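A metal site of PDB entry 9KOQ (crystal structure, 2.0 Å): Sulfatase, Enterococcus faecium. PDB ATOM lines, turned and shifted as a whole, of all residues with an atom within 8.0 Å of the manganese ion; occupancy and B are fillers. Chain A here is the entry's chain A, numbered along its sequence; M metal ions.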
ATOM      1  N   VAL A  14      -7.140   1.284  30.764  1.00  0.00           N
ATOM      2  CA  VAL A  14      -6.510   0.993  29.487  1.00  0.00           C
ATOM      3  C   VAL A  14      -5.982   2.302  28.923  1.00  0.00           C
ATOM      4  O   VAL A  14      -6.677   3.318  28.952  1.00  0.00           O
ATOM      5  CB  VAL A  14      -7.502   0.319  28.504  1.00  0.00           C
ATOM      6  CG1 VAL A  14      -6.794  -0.140  27.239  1.00  0.00           C
ATOM      7  CG2 VAL A  14      -8.200  -0.871  29.181  1.00  0.00           C
ATOM      8  N   VAL A  15      -4.737   2.283  28.435  1.00  0.00           N
ATOM      9  CA  VAL A  15      -4.190   3.390  27.655  1.00  0.00           C
ATOM     10  C   VAL A  15      -3.907   2.850  26.258  1.00  0.00           C
ATOM     11  O   VAL A  15      -3.813   1.642  26.044  1.00  0.00           O
ATOM     12  CB  VAL A  15      -2.902   3.985  28.268  1.00  0.00           C
ATOM     13  CG1 VAL A  15      -3.214   4.642  29.605  1.00  0.00           C
ATOM     14  CG2 VAL A  15      -1.821   2.901  28.428  1.00  0.00           C
ATOM     15  N   ASP A  16      -3.739   3.755  25.312  1.00  0.00           N
ATOM     16  CA  ASP A  16      -3.582   3.350  23.913  1.00  0.00           C
ATOM     17  C   ASP A  16      -2.191   3.710  23.426  1.00  0.00           C
ATOM     18  O   ASP A  16      -1.796   4.873  23.477  1.00  0.00           O
ATOM     19  CB  ASP A  16      -4.644   4.010  23.034  1.00  0.00           C
ATOM     20  CG  ASP A  16      -4.789   3.316  21.696  1.00  0.00           C
ATOM     21  OD1 ASP A  16      -3.748   3.050  21.057  1.00  0.00           O
ATOM     22  OD2 ASP A  16      -5.925   2.956  21.326  1.00  0.00           O
ATOM     23  N   GLN A  17      -1.438   2.701  22.971  1.00  0.00           N
ATOM     24  CA  GLN A  17      -0.152   2.907  22.307  1.00  0.00           C
ATOM     25  C   GLN A  17       0.965   3.286  23.276  1.00  0.00           C
ATOM     26  O   GLN A  17       1.923   3.970  22.894  1.00  0.00           O
ATOM     27  CB  GLN A  17      -0.261   3.966  21.190  1.00  0.00           C
ATOM     28  CG  GLN A  17       0.726   3.770  20.046  1.00  0.00           C
ATOM     29  CD  GLN A  17       0.195   4.261  18.710  1.00  0.00           C
ATOM     30  OE1 GLN A  17      -0.856   3.823  18.266  1.00  0.00           O
ATOM     31  NE2 GLN A  17       0.927   5.163  18.059  1.00  0.00           N
ATOM     32  N   MET A  18       0.892   2.841  24.527  1.00  0.00           N
ATOM     33  CA  MET A  18       1.988   3.062  25.467  1.00  0.00           C
ATOM     34  C   MET A  18       2.946   1.878  25.505  1.00  0.00           C
ATOM     35  O   MET A  18       2.540   0.746  25.731  1.00  0.00           O
ATOM     36  CB  MET A  18       1.418   3.390  26.856  1.00  0.00           C
ATOM     37  CG  MET A  18       2.438   3.895  27.868  1.00  0.00           C
ATOM     38  SD  MET A  18       1.863   3.718  29.559  1.00  0.00           S
ATOM     39  CE  MET A  18       3.359   4.005  30.513  1.00  0.00           C
ATOM     40  N   PRO A  55      -0.244  -6.537  17.400  1.00  0.00           N
ATOM     41  CA  PRO A  55      -0.135  -5.214  18.084  1.00  0.00           C
ATOM     42  C   PRO A  55      -0.689  -4.049  17.266  1.00  0.00           C
ATOM     43  O   PRO A  55       0.050  -3.222  16.711  1.00  0.00           O
ATOM     44  CB  PRO A  55       1.372  -5.082  18.295  1.00  0.00           C
ATOM     45  CG  PRO A  55       1.955  -5.817  17.105  1.00  0.00           C
ATOM     46  CD  PRO A  55       1.048  -6.980  16.845  1.00  0.00           C
ATOM     47  N   SER A  56      -2.020  -3.968  17.193  1.00  0.00           N
ATOM     48  CA  SER A  56      -2.666  -2.732  16.785  1.00  0.00           C
ATOM     49  C   SER A  56      -4.004  -2.685  17.504  1.00  0.00           C
ATOM     50  O   SER A  56      -4.421  -3.644  18.142  1.00  0.00           O
ATOM     51  CB  SER A  56      -2.803  -2.607  15.255  1.00  0.00           C
ATOM     52  OG  SER A  56      -3.612  -3.615  14.700  1.00  0.00           O
ATOM     53  N   CYS A  57      -4.697  -1.548  17.361  1.00  0.00           N
ATOM     54  CA  CYS A  57      -5.813  -1.214  18.257  1.00  0.00           C
ATOM     55  C   CYS A  57      -6.902  -2.280  18.224  1.00  0.00           C
ATOM     56  O   CYS A  57      -7.268  -2.852  19.259  1.00  0.00           O
ATOM     57  CB  CYS A  57      -6.393   0.148  17.875  1.00  0.00           C
ATOM     58  SG  CYS A  57      -5.342   1.568  18.215  1.00  0.00           S
ATOM     59  N   VAL A  58      -7.468  -2.538  17.037  1.00  0.00           N
ATOM     60  CA  VAL A  58      -8.672  -3.360  16.942  1.00  0.00           C
ATOM     61  C   VAL A  58      -8.396  -4.812  17.317  1.00  0.00           C
ATOM     62  O   VAL A  58      -9.124  -5.349  18.169  1.00  0.00           O
ATOM     63  CB  VAL A  58      -9.301  -3.255  15.546  1.00  0.00           C
ATOM     64  CG1 VAL A  58     -10.440  -4.261  15.416  1.00  0.00           C
ATOM     65  CG2 VAL A  58      -9.809  -1.849  15.317  1.00  0.00           C
ATOM     66  N   ALA A  60      -6.018  -5.996  19.197  1.00  0.00           N
ATOM     67  CA  ALA A  60      -5.657  -6.067  20.608  1.00  0.00           C
ATOM     68  C   ALA A  60      -6.881  -5.868  21.504  1.00  0.00           C
ATOM     69  O   ALA A  60      -7.021  -6.532  22.553  1.00  0.00           O
ATOM     70  CB  ALA A  60      -4.580  -5.026  20.929  1.00  0.00           C
ATOM     71  N   ARG A  61      -7.776  -4.960  21.126  1.00  0.00           N
ATOM     72  CA  ARG A  61      -8.945  -4.740  21.970  1.00  0.00           C
ATOM     73  C   ARG A  61      -9.940  -5.892  21.872  1.00  0.00           C
ATOM     74  O   ARG A  61     -10.596  -6.227  22.856  1.00  0.00           O
ATOM     75  CB  ARG A  61      -9.590  -3.395  21.618  1.00  0.00           C
ATOM     76  CG  ARG A  61      -8.732  -2.239  22.152  1.00  0.00           C
ATOM     77  CD  ARG A  61      -9.072  -0.884  21.533  1.00  0.00           C
ATOM     78  NE  ARG A  61      -8.087   0.092  21.969  1.00  0.00           N
ATOM     79  CZ  ARG A  61      -8.118   0.683  23.166  1.00  0.00           C
ATOM     80  NH1 ARG A  61      -9.085   0.431  24.025  1.00  0.00           N
ATOM     81  NH2 ARG A  61      -7.150   1.534  23.501  1.00  0.00           N
ATOM     82  N   TYR A  78      -5.079  -5.101  11.444  1.00  0.00           N
ATOM     83  CA  TYR A  78      -5.996  -3.981  11.666  1.00  0.00           C
ATOM     84  C   TYR A  78      -7.077  -3.969  10.600  1.00  0.00           C
ATOM     85  O   TYR A  78      -6.791  -3.992   9.391  1.00  0.00           O
ATOM     86  CB  TYR A  78      -5.243  -2.657  11.667  1.00  0.00           C
ATOM     87  CG  TYR A  78      -6.126  -1.477  12.048  1.00  0.00           C
ATOM     88  CD1 TYR A  78      -7.015  -0.918  11.138  1.00  0.00           C
ATOM     89  CD2 TYR A  78      -6.114  -0.987  13.352  1.00  0.00           C
ATOM     90  CE1 TYR A  78      -7.839   0.147  11.490  1.00  0.00           C
ATOM     91  CE2 TYR A  78      -6.919   0.072  13.727  1.00  0.00           C
ATOM     92  CZ  TYR A  78      -7.796   0.639  12.800  1.00  0.00           C
ATOM     93  OH  TYR A  78      -8.603   1.685  13.177  1.00  0.00           O
ATOM     94  N   LYS A 106     -12.281   4.906  25.199  1.00  0.00           N
ATOM     95  CA  LYS A 106     -12.107   4.216  23.921  1.00  0.00           C
ATOM     96  C   LYS A 106     -12.541   2.746  24.008  1.00  0.00           C
ATOM     97  O   LYS A 106     -12.018   1.994  24.829  1.00  0.00           O
ATOM     98  CB  LYS A 106     -10.643   4.324  23.465  1.00  0.00           C
ATOM     99  CG  LYS A 106     -10.402   3.675  22.102  1.00  0.00           C
ATOM    100  CD  LYS A 106      -9.056   4.072  21.515  1.00  0.00           C
ATOM    101  CE  LYS A 106      -8.844   3.425  20.139  1.00  0.00           C
ATOM    102  NZ  LYS A 106      -7.575   3.852  19.491  1.00  0.00           N
ATOM    103  N   HIS A 108     -13.464   1.242  20.565  1.00  0.00           N
ATOM    104  CA  HIS A 108     -13.056   0.866  19.211  1.00  0.00           C
ATOM    105  C   HIS A 108     -13.770  -0.393  18.736  1.00  0.00           C
ATOM    106  O   HIS A 108     -13.170  -1.283  18.125  1.00  0.00           O
ATOM    107  CB  HIS A 108     -11.539   0.708  19.080  1.00  0.00           C
ATOM    108  CG  HIS A 108     -11.027   1.008  17.706  1.00  0.00           C
ATOM    109  ND1 HIS A 108      -9.707   1.253  17.424  1.00  0.00           N
ATOM    110  CD2 HIS A 108     -11.685   1.103  16.525  1.00  0.00           C
ATOM    111  CE1 HIS A 108      -9.562   1.499  16.141  1.00  0.00           C
ATOM    112  NE2 HIS A 108     -10.759   1.413  15.568  1.00  0.00           N
ATOM    113  N   PHE A 212      -8.194   5.534  28.120  1.00  0.00           N
ATOM    114  CA  PHE A 212      -7.583   6.740  27.597  1.00  0.00           C
ATOM    115  C   PHE A 212      -7.197   6.571  26.132  1.00  0.00           C
ATOM    116  O   PHE A 212      -6.605   5.568  25.758  1.00  0.00           O
ATOM    117  CB  PHE A 212      -6.331   7.094  28.411  1.00  0.00           C
ATOM    118  CG  PHE A 212      -6.607   7.408  29.859  1.00  0.00           C
ATOM    119  CD1 PHE A 212      -6.569   6.411  30.807  1.00  0.00           C
ATOM    120  CD2 PHE A 212      -6.866   8.699  30.259  1.00  0.00           C
ATOM    121  CE1 PHE A 212      -6.813   6.692  32.144  1.00  0.00           C
ATOM    122  CE2 PHE A 212      -7.126   8.998  31.593  1.00  0.00           C
ATOM    123  CZ  PHE A 212      -7.080   7.991  32.535  1.00  0.00           C
ATOM    124  N   GLU A 213      -7.484   7.587  25.311  1.00  0.00           N
ATOM    125  CA  GLU A 213      -7.032   7.484  23.929  1.00  0.00           C
ATOM    126  C   GLU A 213      -5.543   7.804  23.794  1.00  0.00           C
ATOM    127  O   GLU A 213      -4.909   7.357  22.835  1.00  0.00           O
ATOM    128  CB  GLU A 213      -7.795   8.424  22.985  1.00  0.00           C
ATOM    129  CG  GLU A 213      -7.764   9.894  23.350  1.00  0.00           C
ATOM    130  CD  GLU A 213      -7.637  10.764  22.095  1.00  0.00           C
ATOM    131  OE1 GLU A 213      -6.935  10.302  21.157  1.00  0.00           O
ATOM    132  OE2 GLU A 213      -8.222  11.877  22.031  1.00  0.00           O
ATOM    133  N   HIS A 216      -1.583   7.608  22.270  1.00  0.00           N
ATOM    134  CA  HIS A 216      -1.799   7.590  20.820  1.00  0.00           C
ATOM    135  C   HIS A 216      -1.890   9.011  20.281  1.00  0.00           C
ATOM    136  O   HIS A 216      -2.538   9.871  20.880  1.00  0.00           O
ATOM    137  CB  HIS A 216      -3.086   6.826  20.528  1.00  0.00           C
ATOM    138  CG  HIS A 216      -3.286   6.474  19.086  1.00  0.00           C
ATOM    139  ND1 HIS A 216      -3.422   7.439  18.108  1.00  0.00           N
ATOM    140  CD2 HIS A 216      -3.438   5.286  18.469  1.00  0.00           C
ATOM    141  CE1 HIS A 216      -3.617   6.839  16.940  1.00  0.00           C
ATOM    142  NE2 HIS A 216      -3.639   5.537  17.140  1.00  0.00           N
ATOM    143  N   SER A 306      -1.887  -1.387  28.473  1.00  0.00           N
ATOM    144  CA  SER A 306      -1.936  -0.729  27.174  1.00  0.00           C
ATOM    145  C   SER A 306      -2.305  -1.752  26.104  1.00  0.00           C
ATOM    146  O   SER A 306      -2.019  -2.936  26.244  1.00  0.00           O
ATOM    147  CB  SER A 306      -0.591  -0.097  26.803  1.00  0.00           C
ATOM    148  OG  SER A 306      -0.741   0.611  25.571  1.00  0.00           O
ATOM    149  N   ASP A 307      -2.928  -1.280  25.017  1.00  0.00           N
ATOM    150  CA  ASP A 307      -3.353  -2.223  23.990  1.00  0.00           C
ATOM    151  C   ASP A 307      -2.200  -2.679  23.105  1.00  0.00           C
ATOM    152  O   ASP A 307      -2.238  -3.810  22.606  1.00  0.00           O
ATOM    153  CB  ASP A 307      -4.523  -1.648  23.165  1.00  0.00           C
ATOM    154  CG  ASP A 307      -4.172  -0.398  22.393  1.00  0.00           C
ATOM    155  OD1 ASP A 307      -3.178   0.275  22.715  1.00  0.00           O
ATOM    156  OD2 ASP A 307      -4.911  -0.105  21.419  1.00  0.00           O
ATOM    157  N   HIS A 308      -1.156  -1.879  22.946  1.00  0.00           N
ATOM    158  CA  HIS A 308       0.040  -2.227  22.179  1.00  0.00           C
ATOM    159  C   HIS A 308       1.005  -1.074  22.380  1.00  0.00           C
ATOM    160  O   HIS A 308       0.656  -0.048  22.961  1.00  0.00           O
ATOM    161  CB  HIS A 308      -0.280  -2.410  20.699  1.00  0.00           C
ATOM    162  CG  HIS A 308      -1.001  -1.231  20.142  1.00  0.00           C
ATOM    163  ND1 HIS A 308      -0.362  -0.049  19.855  1.00  0.00           N
ATOM    164  CD2 HIS A 308      -2.317  -1.016  19.929  1.00  0.00           C
ATOM    165  CE1 HIS A 308      -1.250   0.842  19.444  1.00  0.00           C
ATOM    166  NE2 HIS A 308      -2.440   0.288  19.491  1.00  0.00           N
ATOM    167  N   GLY A 309       2.225  -1.217  21.849  1.00  0.00           N
ATOM    168  CA  GLY A 309       3.244  -0.197  21.940  1.00  0.00           C
ATOM    169  C   GLY A 309       3.287   0.757  20.750  1.00  0.00           C
ATOM    170  O   GLY A 309       2.316   0.944  20.016  1.00  0.00           O
ATOM    171  N   LYS A 320       2.896   1.115  14.726  1.00  0.00           N
ATOM    172  CA  LYS A 320       2.892  -0.224  15.317  1.00  0.00           C
ATOM    173  C   LYS A 320       2.536  -1.230  14.235  1.00  0.00           C
ATOM    174  O   LYS A 320       2.637  -0.956  13.036  1.00  0.00           O
ATOM    175  CB  LYS A 320       1.928  -0.276  16.523  1.00  0.00           C
ATOM    176  CG  LYS A 320       0.445  -0.069  16.170  1.00  0.00           C
ATOM    177  CD  LYS A 320       0.042   1.389  16.185  1.00  0.00           C
ATOM    178  CE  LYS A 320      -1.455   1.517  15.958  1.00  0.00           C
ATOM    179  NZ  LYS A 320      -1.844   2.955  15.773  1.00  0.00           N
HETATM  180 MN    MN M   1      -4.305   1.290  19.997  1.00  0.00          MN
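The side-chain sulfur of Cys 57 sits close to the side-chain amino group of Lys 106 (3.4 Å). The guanidinium group (NE) of Arg 61 sits close to the side-chain carboxylate (OD2) of Asp 307 (3.2 Å). The backbone NH (N) of Asp 307 sits at hydrogen-bond distance from the backbone carbonyl oxygen (O) of Val 15, at 3.2 Å. The side-chain amino group (NZ) of Lys 106 lies close to the side-chain carboxylate (OD2) of Asp 16, at 2.6 Å. N of Asp 16 lies within hydrogen-bond range of O of Phe 212. The backbone carbonyl oxygen of His 308 lies close to the backbone NH of Gln 17. The backbone carbonyl oxygen (O) of His 308 sits at hydrogen-bond distance from the side-chain hydroxyl (OG) of Ser 306. N of Met 18 lies within hydrogen-bond range of O of His 308, 3.3 Å away.
Four residues have an atom within 4 Å of the manganese ion: Asp 16, Cys 57, Asp 307 and His 308. The nearest printed residue that does not touch the manganese ion is Lys 106 (4.2 Å).
The manganese ion is bound by the side-chain sulfur (SG) of Cys 57 (2.1 Å), the side-chain carboxylate (OD2) of Asp 307 (2.1 Å), the side-chain carboxylate (OD1) of Asp 16 (2.1 Å), a ring nitrogen (NE2) of His 308 (2.2 Å) and the side-chain carboxylate (OD2) of Asp 16 (2.7 Å). The manganese ion has five donor atoms within binding distance.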
